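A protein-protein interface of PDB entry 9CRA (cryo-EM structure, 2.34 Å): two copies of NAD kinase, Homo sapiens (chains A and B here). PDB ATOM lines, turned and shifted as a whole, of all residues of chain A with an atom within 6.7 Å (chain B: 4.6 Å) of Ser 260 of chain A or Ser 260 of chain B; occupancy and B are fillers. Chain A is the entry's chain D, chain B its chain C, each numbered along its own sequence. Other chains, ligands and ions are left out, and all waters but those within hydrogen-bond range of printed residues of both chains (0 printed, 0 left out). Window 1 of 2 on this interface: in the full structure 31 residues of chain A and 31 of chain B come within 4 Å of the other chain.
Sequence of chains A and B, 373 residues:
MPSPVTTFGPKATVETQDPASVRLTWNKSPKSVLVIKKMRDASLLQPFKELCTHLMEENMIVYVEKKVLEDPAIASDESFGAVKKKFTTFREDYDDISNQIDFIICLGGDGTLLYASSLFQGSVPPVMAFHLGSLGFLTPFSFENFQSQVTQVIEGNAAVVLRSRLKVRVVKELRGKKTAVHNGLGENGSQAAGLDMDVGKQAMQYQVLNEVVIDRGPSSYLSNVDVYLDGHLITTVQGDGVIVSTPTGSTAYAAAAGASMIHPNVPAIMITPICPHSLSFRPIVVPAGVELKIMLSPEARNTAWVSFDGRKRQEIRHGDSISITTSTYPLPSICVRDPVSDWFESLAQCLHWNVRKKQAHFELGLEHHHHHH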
ATOM      1  N   PRO A 247      12.068  21.794  14.557  1.00  0.00           N
ATOM      2  CA  PRO A 247      12.116  20.560  15.361  1.00  0.00           C
ATOM      3  C   PRO A 247      11.129  20.542  16.517  1.00  0.00           C
ATOM      4  O   PRO A 247      10.487  19.511  16.755  1.00  0.00           O
ATOM      5  CB  PRO A 247      13.569  20.527  15.849  1.00  0.00           C
ATOM      6  CG  PRO A 247      14.320  21.232  14.788  1.00  0.00           C
ATOM      7  CD  PRO A 247      13.417  22.333  14.309  1.00  0.00           C
ATOM      8  N   SER A 250       7.899  19.415  15.407  1.00  0.00           N
ATOM      9  CA  SER A 250       7.826  18.110  14.759  1.00  0.00           C
ATOM     10  C   SER A 250       6.688  17.273  15.329  1.00  0.00           C
ATOM     11  O   SER A 250       6.027  16.530  14.595  1.00  0.00           O
ATOM     12  CB  SER A 250       9.159  17.376  14.908  1.00  0.00           C
ATOM     13  OG  SER A 250       9.463  17.148  16.272  1.00  0.00           O
ATOM     14  N   THR A 251       6.448  17.378  16.633  1.00  0.00           N
ATOM     15  CA  THR A 251       5.364  16.666  17.296  1.00  0.00           C
ATOM     16  C   THR A 251       4.039  17.411  17.218  1.00  0.00           C
ATOM     17  O   THR A 251       3.028  16.911  17.720  1.00  0.00           O
ATOM     18  CB  THR A 251       5.727  16.404  18.758  1.00  0.00           C
ATOM     19  OG1 THR A 251       5.820  17.650  19.457  1.00  0.00           O
ATOM     20  CG2 THR A 251       7.060  15.680  18.850  1.00  0.00           C
ATOM     21  N   ALA A 254       2.542  18.930  12.263  1.00  0.00           N
ATOM     22  CA  ALA A 254       3.394  18.150  11.370  1.00  0.00           C
ATOM     23  C   ALA A 254       3.319  16.662  11.690  1.00  0.00           C
ATOM     24  O   ALA A 254       3.254  15.827  10.778  1.00  0.00           O
ATOM     25  CB  ALA A 254       4.838  18.644  11.457  1.00  0.00           C
ATOM     26  N   ALA A 255       3.327  16.306  12.979  1.00  0.00           N
ATOM     27  CA  ALA A 255       3.234  14.901  13.360  1.00  0.00           C
ATOM     28  C   ALA A 255       1.901  14.294  12.952  1.00  0.00           C
ATOM     29  O   ALA A 255       1.826  13.093  12.668  1.00  0.00           O
ATOM     30  CB  ALA A 255       3.436  14.742  14.866  1.00  0.00           C
ATOM     31  N   GLY A 258       2.058  12.871   9.416  1.00  0.00           N
ATOM     32  CA  GLY A 258       2.986  11.789   9.169  1.00  0.00           C
ATOM     33  C   GLY A 258       4.456  12.123   9.311  1.00  0.00           C
ATOM     34  O   GLY A 258       5.295  11.303   8.920  1.00  0.00           O
ATOM     35  N   ALA A 259       4.800  13.288   9.852  1.00  0.00           N
ATOM     36  CA  ALA A 259       6.200  13.636  10.035  1.00  0.00           C
ATOM     37  C   ALA A 259       6.811  12.827  11.176  1.00  0.00           C
ATOM     38  O   ALA A 259       6.121  12.351  12.081  1.00  0.00           O
ATOM     39  CB  ALA A 259       6.353  15.132  10.311  1.00  0.00           C
ATOM     40  N   SER A 260       8.131  12.674  11.120  1.00  0.00           N
ATOM     41  CA  SER A 260       8.857  11.929  12.135  1.00  0.00           C
ATOM     42  C   SER A 260       9.062  12.782  13.385  1.00  0.00           C
ATOM     43  O   SER A 260       8.825  13.993  13.395  1.00  0.00           O
ATOM     44  CB  SER A 260      10.202  11.454  11.589  1.00  0.00           C
ATOM     45  OG  SER A 260      10.028  10.540  10.522  1.00  0.00           O
ATOM     46  N   MET A 261       9.510  12.129  14.453  1.00  0.00           N
ATOM     47  CA  MET A 261       9.788  12.801  15.714  1.00  0.00           C
ATOM     48  C   MET A 261      11.225  13.306  15.689  1.00  0.00           C
ATOM     49  O   MET A 261      12.161  12.519  15.520  1.00  0.00           O
ATOM     50  CB  MET A 261       9.570  11.854  16.893  1.00  0.00           C
ATOM     51  CG  MET A 261       8.217  11.123  16.939  1.00  0.00           C
ATOM     52  SD  MET A 261       6.733  12.089  17.314  1.00  0.00           S
ATOM     53  CE  MET A 261       6.376  12.905  15.762  1.00  0.00           C
ATOM     54  N   ILE A 262      11.401  14.614  15.852  1.00  0.00           N
ATOM     55  CA  ILE A 262      12.709  15.250  15.758  1.00  0.00           C
ATOM     56  C   ILE A 262      13.002  15.987  17.056  1.00  0.00           C
ATOM     57  O   ILE A 262      12.212  16.832  17.491  1.00  0.00           O
ATOM     58  CB  ILE A 262      12.791  16.196  14.546  1.00  0.00           C
ATOM     59  CG1 ILE A 262      12.823  15.385  13.250  1.00  0.00           C
ATOM     60  CG2 ILE A 262      13.993  17.096  14.649  1.00  0.00           C
ATOM     61  CD1 ILE A 262      12.775  16.224  12.005  1.00  0.00           C
ATOM     62  N   MET A 270      11.773  21.090   8.786  1.00  0.00           N
ATOM     63  CA  MET A 270      10.901  20.075   8.219  1.00  0.00           C
ATOM     64  C   MET A 270      10.055  20.656   7.096  1.00  0.00           C
ATOM     65  O   MET A 270       9.727  21.844   7.091  1.00  0.00           O
ATOM     66  CB  MET A 270       9.979  19.488   9.288  1.00  0.00           C
ATOM     67  CG  MET A 270      10.680  18.785  10.428  1.00  0.00           C
ATOM     68  SD  MET A 270       9.658  17.441  11.061  1.00  0.00           S
ATOM     69  CE  MET A 270       9.837  16.238   9.747  1.00  0.00           C
ATOM     70  N   THR A 272       6.498  19.088   5.509  1.00  0.00           N
ATOM     71  CA  THR A 272       5.528  18.013   5.628  1.00  0.00           C
ATOM     72  C   THR A 272       4.238  18.428   4.932  1.00  0.00           C
ATOM     73  O   THR A 272       3.732  19.538   5.176  1.00  0.00           O
ATOM     74  CB  THR A 272       5.259  17.678   7.104  1.00  0.00           C
ATOM     75  OG1 THR A 272       6.482  17.279   7.735  1.00  0.00           O
ATOM     76  CG2 THR A 272       4.245  16.552   7.227  1.00  0.00           C
ATOM     77  N   ARG A 282       6.798  12.027   0.811  1.00  0.00           N
ATOM     78  CA  ARG A 282       7.076  11.921   2.233  1.00  0.00           C
ATOM     79  C   ARG A 282       7.686  13.213   2.765  1.00  0.00           C
ATOM     80  O   ARG A 282       8.312  13.967   2.012  1.00  0.00           O
ATOM     81  CB  ARG A 282       8.022  10.757   2.505  1.00  0.00           C
ATOM     82  CG  ARG A 282       7.303   9.449   2.764  1.00  0.00           C
ATOM     83  CD  ARG A 282       8.233   8.402   3.336  1.00  0.00           C
ATOM     84  NE  ARG A 282       7.804   7.057   2.978  1.00  0.00           N
ATOM     85  CZ  ARG A 282       8.588   5.989   3.012  1.00  0.00           C
ATOM     86  NH1 ARG A 282       9.855   6.074   3.380  1.00  0.00           N
ATOM     87  NH2 ARG A 282       8.087   4.806   2.668  1.00  0.00           N
ATOM     88  N   PRO A 283       7.507  13.494   4.056  1.00  0.00           N
ATOM     89  CA  PRO A 283       8.127  14.688   4.639  1.00  0.00           C
ATOM     90  C   PRO A 283       9.643  14.626   4.534  1.00  0.00           C
ATOM     91  O   PRO A 283      10.248  13.557   4.633  1.00  0.00           O
ATOM     92  CB  PRO A 283       7.657  14.656   6.099  1.00  0.00           C
ATOM     93  CG  PRO A 283       7.267  13.233   6.344  1.00  0.00           C
ATOM     94  CD  PRO A 283       6.705  12.754   5.046  1.00  0.00           C
ATOM     95  N   ILE A 284      10.254  15.789   4.327  1.00  0.00           N
ATOM     96  CA  ILE A 284      11.694  15.878   4.144  1.00  0.00           C
ATOM     97  C   ILE A 284      12.283  16.766   5.230  1.00  0.00           C
ATOM     98  O   ILE A 284      11.608  17.622   5.810  1.00  0.00           O
ATOM     99  CB  ILE A 284      12.079  16.404   2.745  1.00  0.00           C
ATOM    100  CG1 ILE A 284      11.551  17.823   2.539  1.00  0.00           C
ATOM    101  CG2 ILE A 284      11.543  15.481   1.665  1.00  0.00           C
ATOM    102  CD1 ILE A 284      11.755  18.349   1.136  1.00  0.00           C
ATOM    103  N   VAL A 285      13.562  16.540   5.511  1.00  0.00           N
ATOM    104  CA  VAL A 285      14.314  17.296   6.504  1.00  0.00           C
ATOM    105  C   VAL A 285      15.493  17.950   5.801  1.00  0.00           C
ATOM    106  O   VAL A 285      16.277  17.267   5.131  1.00  0.00           O
ATOM    107  CB  VAL A 285      14.789  16.396   7.660  1.00  0.00           C
ATOM    108  CG1 VAL A 285      15.392  17.230   8.766  1.00  0.00           C
ATOM    109  CG2 VAL A 285      13.636  15.560   8.191  1.00  0.00           C
ATOM    110  N   SER B 250      18.968   7.568   5.277  1.00  0.00           N
ATOM    111  CA  SER B 250      17.571   7.982   5.380  1.00  0.00           C
ATOM    112  C   SER B 250      16.757   7.515   4.183  1.00  0.00           C
ATOM    113  O   SER B 250      15.571   7.202   4.325  1.00  0.00           O
ATOM    114  CB  SER B 250      17.484   9.501   5.515  1.00  0.00           C
ATOM    115  OG  SER B 250      17.934  10.143   4.334  1.00  0.00           O
ATOM    116  N   GLY B 258       9.246   3.514   6.419  1.00  0.00           N
ATOM    117  CA  GLY B 258       8.448   4.693   6.684  1.00  0.00           C
ATOM    118  C   GLY B 258       9.199   5.891   7.222  1.00  0.00           C
ATOM    119  O   GLY B 258       8.558   6.867   7.626  1.00  0.00           O
ATOM    120  N   ALA B 259      10.527   5.854   7.242  1.00  0.00           N
ATOM    121  CA  ALA B 259      11.297   6.983   7.739  1.00  0.00           C
ATOM    122  C   ALA B 259      11.238   8.154   6.762  1.00  0.00           C
ATOM    123  O   ALA B 259      10.985   7.985   5.566  1.00  0.00           O
ATOM    124  CB  ALA B 259      12.746   6.571   7.981  1.00  0.00           C
ATOM    125  N   SER B 260      11.471   9.353   7.289  1.00  0.00           N
ATOM    126  CA  SER B 260      11.426  10.566   6.488  1.00  0.00           C
ATOM    127  C   SER B 260      12.708  10.716   5.670  1.00  0.00           C
ATOM    128  O   SER B 260      13.624   9.891   5.731  1.00  0.00           O
ATOM    129  CB  SER B 260      11.208  11.783   7.382  1.00  0.00           C
ATOM    130  OG  SER B 260      10.137  11.568   8.282  1.00  0.00           O
ATOM    131  N   MET B 261      12.770  11.792   4.890  1.00  0.00           N
ATOM    132  CA  MET B 261      13.919  12.097   4.047  1.00  0.00           C
ATOM    133  C   MET B 261      14.764  13.153   4.749  1.00  0.00           C
ATOM    134  O   MET B 261      14.274  14.250   5.036  1.00  0.00           O
ATOM    135  CB  MET B 261      13.464  12.602   2.678  1.00  0.00           C
ATOM    136  CG  MET B 261      12.707  11.589   1.828  1.00  0.00           C
ATOM    137  SD  MET B 261      13.640  10.114   1.395  1.00  0.00           S
ATOM    138  CE  MET B 261      12.957   8.933   2.551  1.00  0.00           C
ATOM    139  N   ILE B 262      16.024  12.829   5.028  1.00  0.00           N
ATOM    140  CA  ILE B 262      16.936  13.746   5.700  1.00  0.00           C
ATOM    141  C   ILE B 262      18.137  14.004   4.801  1.00  0.00           C
ATOM    142  O   ILE B 262      18.783  13.060   4.330  1.00  0.00           O
ATOM    143  CB  ILE B 262      17.380  13.212   7.075  1.00  0.00           C
ATOM    144  CG1 ILE B 262      16.160  12.827   7.912  1.00  0.00           C
ATOM    145  CG2 ILE B 262      18.218  14.244   7.801  1.00  0.00           C
ATOM    146  CD1 ILE B 262      16.497  12.341   9.299  1.00  0.00           C
ATOM    147  N   MET B 270      19.165   8.550  13.236  1.00  0.00           N
ATOM    148  CA  MET B 270      17.789   8.126  13.034  1.00  0.00           C
ATOM    149  C   MET B 270      17.511   6.843  13.804  1.00  0.00           C
ATOM    150  O   MET B 270      18.420   6.051  14.065  1.00  0.00           O
ATOM    151  CB  MET B 270      17.511   7.912  11.549  1.00  0.00           C
ATOM    152  CG  MET B 270      17.569   9.188  10.743  1.00  0.00           C
ATOM    153  SD  MET B 270      17.323   8.892   8.990  1.00  0.00           S
ATOM    154  CE  MET B 270      15.591   8.465   8.989  1.00  0.00           C
ATOM    155  N   ARG B 282       6.238   5.939  15.966  1.00  0.00           N
ATOM    156  CA  ARG B 282       6.729   6.748  14.863  1.00  0.00           C
ATOM    157  C   ARG B 282       8.257   6.781  14.879  1.00  0.00           C
ATOM    158  O   ARG B 282       8.866   6.805  15.953  1.00  0.00           O
ATOM    159  CB  ARG B 282       6.171   8.168  14.965  1.00  0.00           C
ATOM    160  CG  ARG B 282       6.263   8.992  13.693  1.00  0.00           C
ATOM    161  CD  ARG B 282       5.289   8.504  12.636  1.00  0.00           C
ATOM    162  NE  ARG B 282       3.899   8.675  13.040  1.00  0.00           N
ATOM    163  CZ  ARG B 282       3.180   9.765  12.811  1.00  0.00           C
ATOM    164  NH1 ARG B 282       3.703  10.822  12.210  1.00  0.00           N
ATOM    165  NH2 ARG B 282       1.908   9.797  13.195  1.00  0.00           N
ATOM    166  N   PRO B 283       8.903   6.770  13.711  1.00  0.00           N
ATOM    167  CA  PRO B 283      10.364   6.913  13.683  1.00  0.00           C
ATOM    168  C   PRO B 283      10.800   8.242  14.281  1.00  0.00           C
ATOM    169  O   PRO B 283      10.120   9.262  14.150  1.00  0.00           O
ATOM    170  CB  PRO B 283      10.706   6.831  12.189  1.00  0.00           C
ATOM    171  CG  PRO B 283       9.409   6.992  11.464  1.00  0.00           C
ATOM    172  CD  PRO B 283       8.348   6.490  12.379  1.00  0.00           C
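NH1 of Arg 282 of chain A sits at hydrogen-bond distance from O of Ala 259 of chain B.
OG of Ser 260 of chain B sits at hydrogen-bond distance from OG of Ser 260 of chain A, at 2.5 Å.
The backbone carbonyl oxygen (O) of Pro 283 of chain A is in hydrogen-bond range of the backbone NH (N) of Met 261 of chain B, 3.1 Å away.
The backbone carbonyl oxygen (O) of Met 261 of chain B lies within hydrogen-bond range of the backbone NH (N) of Val 285 of chain A (2.4 Å).
The guanidinium group (NH1) of Arg 282 of chain B is in hydrogen-bond range of the backbone carbonyl oxygen (O) of Ala 255 of chain A (3.0 Å).
The guanidinium group (NH1) of Arg 282 of chain B is in hydrogen-bond range of the backbone carbonyl oxygen (O) of Ala 259 of chain A (2.9 Å).
The backbone NH (N) of Met 261 of chain A sits at hydrogen-bond distance from the backbone carbonyl oxygen (O) of Pro 283 of chain B (2.9 Å).
The side-chain hydroxyl of Ser 250 of chain B lies within hydrogen-bond range of the backbone carbonyl oxygen of Ile 262 of chain B.
N of Ala 255 of chain A sits at hydrogen-bond distance from O of Ser 250 of chain A, at 3.2 Å.
The backbone carbonyl oxygen of Ala 254 of chain A lies within hydrogen-bond range of the backbone NH of Ala 259 of chain A (3.1 Å).
Among the printed residues, pairs that only touch across the chains: Ile 284 of chain A with Met 261 of chain B (3.2 Å), Gly 258 of chain A with Arg 282 of chain B (3.3 Å), Ser 260 of chain A with Pro 283 of chain B (3.4 Å), Pro 283 of chain A with Ser 260 of chain B (3.4 Å), Val 285 of chain A with Ile 262 of chain B (3.6 Å) and Arg 282 of chain A with Gly 258 of chain B (3.8 Å).
Of chain B, only Ser 260 and Pro 283 come within 4 Å of Ser 260 of chain A.
Of chain A, only Ser 260 (2.5 Å) and Pro 283 (3.4 Å) come within 4 Å of Ser 260 of chain B.
Of the printed residues of chain A, Met 261 of chain B touches Pro 283 (3.1 Å), Ile 284 (3.2 Å) and Val 285 (2.4 Å).
Printed residues of chain B within 4 Å of Ala 255 of chain A: Arg 282 (3.0 Å).
Printed residues of chain A within 4 Å of Ile 262 of chain B: Val 285 (3.6 Å).
Printed residues of chain B within 4 Å of Ile 284 of chain A: Met 261 (3.2 Å).
Printed residues of chain B within 4 Å of Pro 283 of chain A: Ser 260 (3.4 Å) and Met 261 (3.1 Å).
Ile 262 of chain A touches none of the printed residues of chain B.
Thr 251 of chain A touches none of the printed residues of chain B.
The nearest residue of chain B that does not touch Ser 260 of chain A is Arg 282 of chain B (4.2 Å).
Of the 16 printed residues of chain A, 9 touch a printed residue of chain B.
Of the 9 printed residues of chain B, 7 touch a printed residue of chain A.
Hydrophobic or aromatic side chains of chain B that line the printed part of chain A: Met 261, Ile 262 and Pro 283.
Along chain B the printed residues that touch a printed residue of chain A span positions 258 to 283.
Among the printed residues, 13 pairs touch across the chains.
Gly 258 of chain A touches Arg 282 of chain B, and with the chains exchanged Arg 282 of chain A touches Gly 258 of chain B.
Ala 259 of chain A touches Arg 282 of chain B, and with the chains exchanged Arg 282 of chain A touches Ala 259 of chain B.
Ser 260 of chain A touches its own counterpart, Ser 260 of chain B.
Met 261 of chain A touches Pro 283 of chain B, and with the chains exchanged Pro 283 of chain A touches Met 261 of chain B.
Positions printed for both chains: 250, 258, 259, 260, 261, 262, 270, 282 and 283.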
